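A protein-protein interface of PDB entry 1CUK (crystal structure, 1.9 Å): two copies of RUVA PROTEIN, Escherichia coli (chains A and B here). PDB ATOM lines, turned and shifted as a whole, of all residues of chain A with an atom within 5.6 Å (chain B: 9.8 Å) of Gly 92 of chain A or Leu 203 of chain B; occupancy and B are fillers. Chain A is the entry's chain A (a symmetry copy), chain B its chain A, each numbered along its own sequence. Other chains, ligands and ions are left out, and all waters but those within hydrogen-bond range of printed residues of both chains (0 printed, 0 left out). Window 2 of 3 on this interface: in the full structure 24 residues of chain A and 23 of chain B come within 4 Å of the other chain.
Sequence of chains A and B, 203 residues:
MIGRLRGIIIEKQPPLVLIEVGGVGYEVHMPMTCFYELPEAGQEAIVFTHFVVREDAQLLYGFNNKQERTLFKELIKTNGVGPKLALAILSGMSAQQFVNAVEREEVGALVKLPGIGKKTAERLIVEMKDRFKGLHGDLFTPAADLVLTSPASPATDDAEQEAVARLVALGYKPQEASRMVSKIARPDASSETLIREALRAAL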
ATOM      1  N   THR A  33     -27.846  11.053   5.081  1.00  0.00           N
ATOM      2  CA  THR A  33     -28.272  10.933   3.722  1.00  0.00           C
ATOM      3  C   THR A  33     -28.854  12.218   3.182  1.00  0.00           C
ATOM      4  O   THR A  33     -28.796  12.455   1.984  1.00  0.00           O
ATOM      5  CB  THR A  33     -29.082   9.690   3.397  1.00  0.00           C
ATOM      6  OG1 THR A  33     -30.336   9.732   4.064  1.00  0.00           O
ATOM      7  CG2 THR A  33     -28.273   8.441   3.769  1.00  0.00           C
ATOM      8  N   LEU A  87     -32.819   9.333  13.334  1.00  0.00           N
ATOM      9  CA  LEU A  87     -31.761  10.013  12.608  1.00  0.00           C
ATOM     10  C   LEU A  87     -30.646   9.044  12.220  1.00  0.00           C
ATOM     11  O   LEU A  87     -30.030   9.168  11.168  1.00  0.00           O
ATOM     12  CB  LEU A  87     -31.200  11.182  13.424  1.00  0.00           C
ATOM     13  CG  LEU A  87     -30.239  12.068  12.638  1.00  0.00           C
ATOM     14  CD1 LEU A  87     -30.583  13.518  12.873  1.00  0.00           C
ATOM     15  CD2 LEU A  87     -28.827  11.831  13.127  1.00  0.00           C
ATOM     16  N   ALA A  88     -30.378   8.062  13.085  1.00  0.00           N
ATOM     17  CA  ALA A  88     -29.339   7.076  12.789  1.00  0.00           C
ATOM     18  C   ALA A  88     -29.812   6.139  11.674  1.00  0.00           C
ATOM     19  O   ALA A  88     -29.057   5.834  10.734  1.00  0.00           O
ATOM     20  CB  ALA A  88     -28.811   6.365  14.039  1.00  0.00           C
ATOM     21  N   ILE A  89     -31.085   5.719  11.727  1.00  0.00           N
ATOM     22  CA  ILE A  89     -31.599   4.863  10.661  1.00  0.00           C
ATOM     23  C   ILE A  89     -31.458   5.517   9.254  1.00  0.00           C
ATOM     24  O   ILE A  89     -31.083   4.891   8.271  1.00  0.00           O
ATOM     25  CB  ILE A  89     -33.029   4.551  10.929  1.00  0.00           C
ATOM     26  CG1 ILE A  89     -33.096   3.590  12.082  1.00  0.00           C
ATOM     27  CG2 ILE A  89     -33.669   3.918   9.707  1.00  0.00           C
ATOM     28  CD1 ILE A  89     -34.461   3.611  12.732  1.00  0.00           C
ATOM     29  N   LEU A  90     -31.768   6.792   9.175  1.00  0.00           N
ATOM     30  CA  LEU A  90     -31.695   7.539   7.932  1.00  0.00           C
ATOM     31  C   LEU A  90     -30.299   8.092   7.611  1.00  0.00           C
ATOM     32  O   LEU A  90     -30.107   8.803   6.626  1.00  0.00           O
ATOM     33  CB  LEU A  90     -32.742   8.645   7.893  1.00  0.00           C
ATOM     34  CG  LEU A  90     -34.114   8.045   7.856  1.00  0.00           C
ATOM     35  CD1 LEU A  90     -35.178   9.157   7.863  1.00  0.00           C
ATOM     36  CD2 LEU A  90     -34.236   7.190   6.614  1.00  0.00           C
ATOM     37  N   SER A  91     -29.316   7.720   8.409  1.00  0.00           N
ATOM     38  CA  SER A  91     -27.963   8.121   8.163  1.00  0.00           C
ATOM     39  C   SER A  91     -27.245   6.911   7.577  1.00  0.00           C
ATOM     40  O   SER A  91     -26.285   7.042   6.845  1.00  0.00           O
ATOM     41  CB  SER A  91     -27.236   8.567   9.382  1.00  0.00           C
ATOM     42  OG  SER A  91     -27.963   9.603   9.953  1.00  0.00           O
ATOM     43  N   GLY A  92     -27.732   5.716   7.931  1.00  0.00           N
ATOM     44  CA  GLY A  92     -27.156   4.460   7.438  1.00  0.00           C
ATOM     45  C   GLY A  92     -27.747   4.116   6.069  1.00  0.00           C
ATOM     46  O   GLY A  92     -27.093   3.561   5.182  1.00  0.00           O
ATOM     47  N   MET A  93     -29.005   4.466   5.905  1.00  0.00           N
ATOM     48  CA  MET A  93     -29.677   4.233   4.657  1.00  0.00           C
ATOM     49  C   MET A  93     -30.562   5.379   4.279  1.00  0.00           C
ATOM     50  O   MET A  93     -30.955   6.180   5.150  1.00  0.00           O
ATOM     51  CB  MET A  93     -30.382   2.888   4.525  1.00  0.00           C
ATOM     52  CG  MET A  93     -31.473   2.587   5.524  1.00  0.00           C
ATOM     53  SD  MET A  93     -32.196   0.937   5.188  1.00  0.00           S
ATOM     54  CE  MET A  93     -30.708  -0.072   5.400  1.00  0.00           C
ATOM     55  N   SER A  94     -30.858   5.473   2.968  1.00  0.00           N
ATOM     56  CA  SER A  94     -31.716   6.535   2.437  1.00  0.00           C
ATOM     57  C   SER A  94     -33.195   6.184   2.626  1.00  0.00           C
ATOM     58  O   SER A  94     -33.531   5.024   2.836  1.00  0.00           O
ATOM     59  CB  SER A  94     -31.391   6.883   0.992  1.00  0.00           C
ATOM     60  OG  SER A  94     -31.949   5.897   0.127  1.00  0.00           O
ATOM     61  N   GLN A  97     -34.210   3.276   0.344  1.00  0.00           N
ATOM     62  CA  GLN A  97     -33.681   1.979   0.776  1.00  0.00           C
ATOM     63  C   GLN A  97     -34.429   1.487   2.010  1.00  0.00           C
ATOM     64  O   GLN A  97     -34.715   0.289   2.143  1.00  0.00           O
ATOM     65  CB  GLN A  97     -32.212   2.115   1.123  1.00  0.00           C
ATOM     66  CG  GLN A  97     -31.382   2.622  -0.049  1.00  0.00           C
ATOM     67  CD  GLN A  97     -29.895   2.643   0.267  1.00  0.00           C
ATOM     68  OE1 GLN A  97     -29.091   2.185  -0.543  1.00  0.00           O
ATOM     69  NE2 GLN A  97     -29.482   3.151   1.411  1.00  0.00           N
ATOM     70  N   ALA A 109     -30.340  -6.196   7.605  1.00  0.00           N
ATOM     71  CA  ALA A 109     -29.856  -4.835   7.432  1.00  0.00           C
ATOM     72  C   ALA A 109     -30.105  -3.918   8.636  1.00  0.00           C
ATOM     73  O   ALA A 109     -29.203  -3.241   9.127  1.00  0.00           O
ATOM     74  CB  ALA A 109     -30.467  -4.244   6.180  1.00  0.00           C
ATOM     75  N   LYS A 112     -27.826  -4.235  11.814  1.00  0.00           N
ATOM     76  CA  LYS A 112     -26.492  -3.689  11.619  1.00  0.00           C
ATOM     77  C   LYS A 112     -26.392  -2.247  12.170  1.00  0.00           C
ATOM     78  O   LYS A 112     -25.385  -1.563  11.982  1.00  0.00           O
ATOM     79  CB  LYS A 112     -26.126  -3.733  10.141  1.00  0.00           C
ATOM     80  CG  LYS A 112     -26.367  -5.102   9.518  1.00  0.00           C
ATOM     81  CD  LYS A 112     -25.246  -5.529   8.580  1.00  0.00           C
ATOM     82  CE  LYS A 112     -24.206  -6.435   9.249  1.00  0.00           C
ATOM     83  NZ  LYS A 112     -23.014  -6.683   8.413  1.00  0.00           N
ATOM     84  N   LEU A 113     -27.466  -1.822  12.880  1.00  0.00           N
ATOM     85  CA  LEU A 113     -27.584  -0.481  13.451  1.00  0.00           C
ATOM     86  C   LEU A 113     -27.630  -0.409  14.961  1.00  0.00           C
ATOM     87  O   LEU A 113     -28.427  -1.071  15.630  1.00  0.00           O
ATOM     88  CB  LEU A 113     -28.796   0.245  12.882  1.00  0.00           C
ATOM     89  CG  LEU A 113     -28.560   0.677  11.459  1.00  0.00           C
ATOM     90  CD1 LEU A 113     -29.837   0.571  10.633  1.00  0.00           C
ATOM     91  CD2 LEU A 113     -28.062   2.104  11.487  1.00  0.00           C
ATOM     92  N   LEU B 167     -20.060   9.937  13.768  1.00  0.00           N
ATOM     93  CA  LEU B 167     -20.373   8.518  13.904  1.00  0.00           C
ATOM     94  C   LEU B 167     -20.761   8.214  15.343  1.00  0.00           C
ATOM     95  O   LEU B 167     -21.547   7.300  15.615  1.00  0.00           O
ATOM     96  CB  LEU B 167     -19.180   7.675  13.499  1.00  0.00           C
ATOM     97  CG  LEU B 167     -19.060   7.546  11.985  1.00  0.00           C
ATOM     98  CD1 LEU B 167     -17.741   6.910  11.553  1.00  0.00           C
ATOM     99  CD2 LEU B 167     -20.173   6.694  11.370  1.00  0.00           C
ATOM    100  N   LEU B 170     -24.120   9.429  16.010  1.00  0.00           N
ATOM    101  CA  LEU B 170     -25.035   8.435  15.445  1.00  0.00           C
ATOM    102  C   LEU B 170     -25.451   7.343  16.421  1.00  0.00           C
ATOM    103  O   LEU B 170     -26.575   6.831  16.356  1.00  0.00           O
ATOM    104  CB  LEU B 170     -24.534   7.856  14.111  1.00  0.00           C
ATOM    105  CG  LEU B 170     -24.453   8.927  13.042  1.00  0.00           C
ATOM    106  CD1 LEU B 170     -24.243   8.299  11.671  1.00  0.00           C
ATOM    107  CD2 LEU B 170     -25.739   9.741  13.079  1.00  0.00           C
ATOM    108  N   TYR B 172     -22.679   5.118  17.726  1.00  0.00           N
ATOM    109  CA  TYR B 172     -21.542   4.265  17.810  1.00  0.00           C
ATOM    110  C   TYR B 172     -20.684   4.588  18.979  1.00  0.00           C
ATOM    111  O   TYR B 172     -20.444   5.761  19.267  1.00  0.00           O
ATOM    112  CB  TYR B 172     -20.700   4.390  16.572  1.00  0.00           C
ATOM    113  CG  TYR B 172     -21.325   3.660  15.458  1.00  0.00           C
ATOM    114  CD1 TYR B 172     -21.354   2.268  15.485  1.00  0.00           C
ATOM    115  CD2 TYR B 172     -21.901   4.338  14.385  1.00  0.00           C
ATOM    116  CE1 TYR B 172     -21.936   1.549  14.445  1.00  0.00           C
ATOM    117  CE2 TYR B 172     -22.485   3.634  13.334  1.00  0.00           C
ATOM    118  CZ  TYR B 172     -22.500   2.238  13.373  1.00  0.00           C
ATOM    119  OH  TYR B 172     -23.073   1.534  12.353  1.00  0.00           O
ATOM    120  N   MET B 180     -13.611   2.439  13.046  1.00  0.00           N
ATOM    121  CA  MET B 180     -14.376   2.370  11.794  1.00  0.00           C
ATOM    122  C   MET B 180     -13.769   3.309  10.731  1.00  0.00           C
ATOM    123  O   MET B 180     -13.744   2.992   9.535  1.00  0.00           O
ATOM    124  CB  MET B 180     -15.837   2.768  12.040  1.00  0.00           C
ATOM    125  CG  MET B 180     -16.434   2.134  13.303  1.00  0.00           C
ATOM    126  SD  MET B 180     -18.211   2.247  13.371  1.00  0.00           S
ATOM    127  CE  MET B 180     -18.882   2.312  11.722  1.00  0.00           C
ATOM    128  N   ILE B 195     -17.382   9.555   6.708  1.00  0.00           N
ATOM    129  CA  ILE B 195     -18.617   9.142   7.381  1.00  0.00           C
ATOM    130  C   ILE B 195     -19.438   8.242   6.496  1.00  0.00           C
ATOM    131  O   ILE B 195     -19.956   7.203   6.896  1.00  0.00           O
ATOM    132  CB  ILE B 195     -19.440  10.336   7.796  1.00  0.00           C
ATOM    133  CG1 ILE B 195     -18.655  11.164   8.789  1.00  0.00           C
ATOM    134  CG2 ILE B 195     -20.718   9.858   8.458  1.00  0.00           C
ATOM    135  CD1 ILE B 195     -19.546  11.952   9.749  1.00  0.00           C
ATOM    136  N   ARG B 196     -19.543   8.666   5.281  1.00  0.00           N
ATOM    137  CA  ARG B 196     -20.263   7.945   4.308  1.00  0.00           C
ATOM    138  C   ARG B 196     -19.723   6.539   4.191  1.00  0.00           C
ATOM    139  O   ARG B 196     -20.441   5.558   4.415  1.00  0.00           O
ATOM    140  CB  ARG B 196     -20.123   8.644   2.992  1.00  0.00           C
ATOM    141  CG  ARG B 196     -20.881   7.911   1.916  1.00  0.00           C
ATOM    142  CD  ARG B 196     -20.768   8.599   0.567  1.00  0.00           C
ATOM    143  NE  ARG B 196     -21.291   9.962   0.586  1.00  0.00           N
ATOM    144  CZ  ARG B 196     -21.308  10.782  -0.476  1.00  0.00           C
ATOM    145  NH1 ARG B 196     -20.831  10.402  -1.675  1.00  0.00           N
ATOM    146  NH2 ARG B 196     -21.823  12.009  -0.335  1.00  0.00           N
ATOM    147  N   GLU B 197     -18.425   6.474   3.829  1.00  0.00           N
ATOM    148  CA  GLU B 197     -17.689   5.210   3.661  1.00  0.00           C
ATOM    149  C   GLU B 197     -17.837   4.297   4.882  1.00  0.00           C
ATOM    150  O   GLU B 197     -18.265   3.129   4.791  1.00  0.00           O
ATOM    151  CB  GLU B 197     -16.214   5.492   3.376  1.00  0.00           C
ATOM    152  N   ALA B 198     -17.474   4.852   6.024  1.00  0.00           N
ATOM    153  CA  ALA B 198     -17.557   4.153   7.262  1.00  0.00           C
ATOM    154  C   ALA B 198     -18.893   3.428   7.397  1.00  0.00           C
ATOM    155  O   ALA B 198     -18.964   2.257   7.745  1.00  0.00           O
ATOM    156  CB  ALA B 198     -17.373   5.147   8.390  1.00  0.00           C
ATOM    157  N   LEU B 199     -19.965   4.142   7.127  1.00  0.00           N
ATOM    158  CA  LEU B 199     -21.259   3.542   7.245  1.00  0.00           C
ATOM    159  C   LEU B 199     -21.457   2.345   6.359  1.00  0.00           C
ATOM    160  O   LEU B 199     -21.782   1.280   6.851  1.00  0.00           O
ATOM    161  CB  LEU B 199     -22.403   4.550   7.177  1.00  0.00           C
ATOM    162  CG  LEU B 199     -22.257   5.605   8.255  1.00  0.00           C
ATOM    163  CD1 LEU B 199     -23.144   6.772   7.907  1.00  0.00           C
ATOM    164  CD2 LEU B 199     -22.665   5.028   9.595  1.00  0.00           C
ATOM    165  N   ARG B 200     -21.249   2.518   5.059  1.00  0.00           N
ATOM    166  CA  ARG B 200     -21.413   1.411   4.110  1.00  0.00           C
ATOM    167  C   ARG B 200     -20.705   0.144   4.575  1.00  0.00           C
ATOM    168  O   ARG B 200     -21.267  -0.952   4.603  1.00  0.00           O
ATOM    169  CB  ARG B 200     -20.957   1.808   2.706  1.00  0.00           C
ATOM    170  N   ALA B 201     -19.459   0.324   4.948  1.00  0.00           N
ATOM    171  CA  ALA B 201     -18.636  -0.751   5.400  1.00  0.00           C
ATOM    172  C   ALA B 201     -19.026  -1.286   6.761  1.00  0.00           C
ATOM    173  O   ALA B 201     -18.279  -2.043   7.360  1.00  0.00           O
ATOM    174  CB  ALA B 201     -17.186  -0.293   5.408  1.00  0.00           C
ATOM    175  N   ALA B 202     -20.169  -0.904   7.277  1.00  0.00           N
ATOM    176  CA  ALA B 202     -20.511  -1.424   8.582  1.00  0.00           C
ATOM    177  C   ALA B 202     -21.923  -1.974   8.645  1.00  0.00           C
ATOM    178  O   ALA B 202     -22.322  -2.630   9.626  1.00  0.00           O
ATOM    179  CB  ALA B 202     -20.223  -0.392   9.662  1.00  0.00           C
ATOM    180  N   LEU B 203     -22.669  -1.694   7.569  1.00  0.00           N
ATOM    181  CA  LEU B 203     -24.049  -2.124   7.422  1.00  0.00           C
ATOM    182  C   LEU B 203     -24.310  -2.746   6.045  1.00  0.00           C
ATOM    183  O   LEU B 203     -23.384  -2.740   5.194  1.00  0.00           O
ATOM    184  CB  LEU B 203     -25.046  -0.970   7.724  1.00  0.00           C
ATOM    185  CG  LEU B 203     -24.767   0.289   6.894  1.00  0.00           C
ATOM    186  CD1 LEU B 203     -25.500   0.208   5.557  1.00  0.00           C
ATOM    187  CD2 LEU B 203     -25.183   1.548   7.656  1.00  0.00           C
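No position is printed for both chains. Of the 8 pairs that touch across the chains among the printed residues, none has its exchanged pair printed and touching as well.
Of the printed residues of chain B, Leu 87 of chain A touches Leu 170. Leu 90 of chain A touches none of the printed residues of chain B. Of the printed residues of chain B, Ser 91 of chain A touches Leu 170 and Leu 199. Of chain B, only Leu 203 comes within 4 Å of Gly 92 of chain A. No residue of chain B comes within 4 Å of Met 93 of chain A. Of the printed residues of chain B, Lys 112 of chain A touches Tyr 172 (3.9 Å), Ala 202 (3.99 Å) and Leu 203 (3.8 Å). Printed residues of chain A within 4 Å of Leu 199 of chain B: Ser 91 (3.3 Å). Printed residues of chain A within 4 Å of Leu 203 of chain B: Gly 92 (3.5 Å) and Lys 112 (3.8 Å). The nearest residue of chain B that does not touch Gly 92 of chain A is Leu 199 of chain B (4.7 Å). The nearest residue of chain A that does not touch Leu 203 of chain B is Leu 113 of chain A (4.8 Å). The nearest printed residue of chain B that does not touch Lys 112 of chain A is Ala 201 of chain B (6.7 Å).
Of the 13 printed residues of chain A, 5 touch a printed residue of chain B. Hydrophobic or aromatic side chains of chain A within 4 Å of the printed part of chain B: Leu 87 and Ala 88. Among the printed residues, 8 pairs touch across the chains.
Among the printed residues, pairs that only touch across the chains: Leu 87 of chain A with Leu 170 of chain B (3.7 Å), Ala 88 of chain A with Leu 170 of chain B (3.3 Å), Ser 91 of chain A with Leu 170 of chain B (3.8 Å), Ser 91 of chain A with Leu 199 of chain B (3.3 Å), Gly 92 of chain A with Leu 203 of chain B (3.5 Å), Lys 112 of chain A with Tyr 172 of chain B (3.9 Å), Lys 112 of chain A with Ala 202 of chain B (3.99 Å) and Lys 112 of chain A with Leu 203 of chain B (3.8 Å).
O of Leu 167 of chain B sits close to N of Tyr 172 of chain B, at 3.2 Å. O of Leu 87 of chain A sits at hydrogen-bond distance from OG of Ser 91 of chain A, at 2.4 Å.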
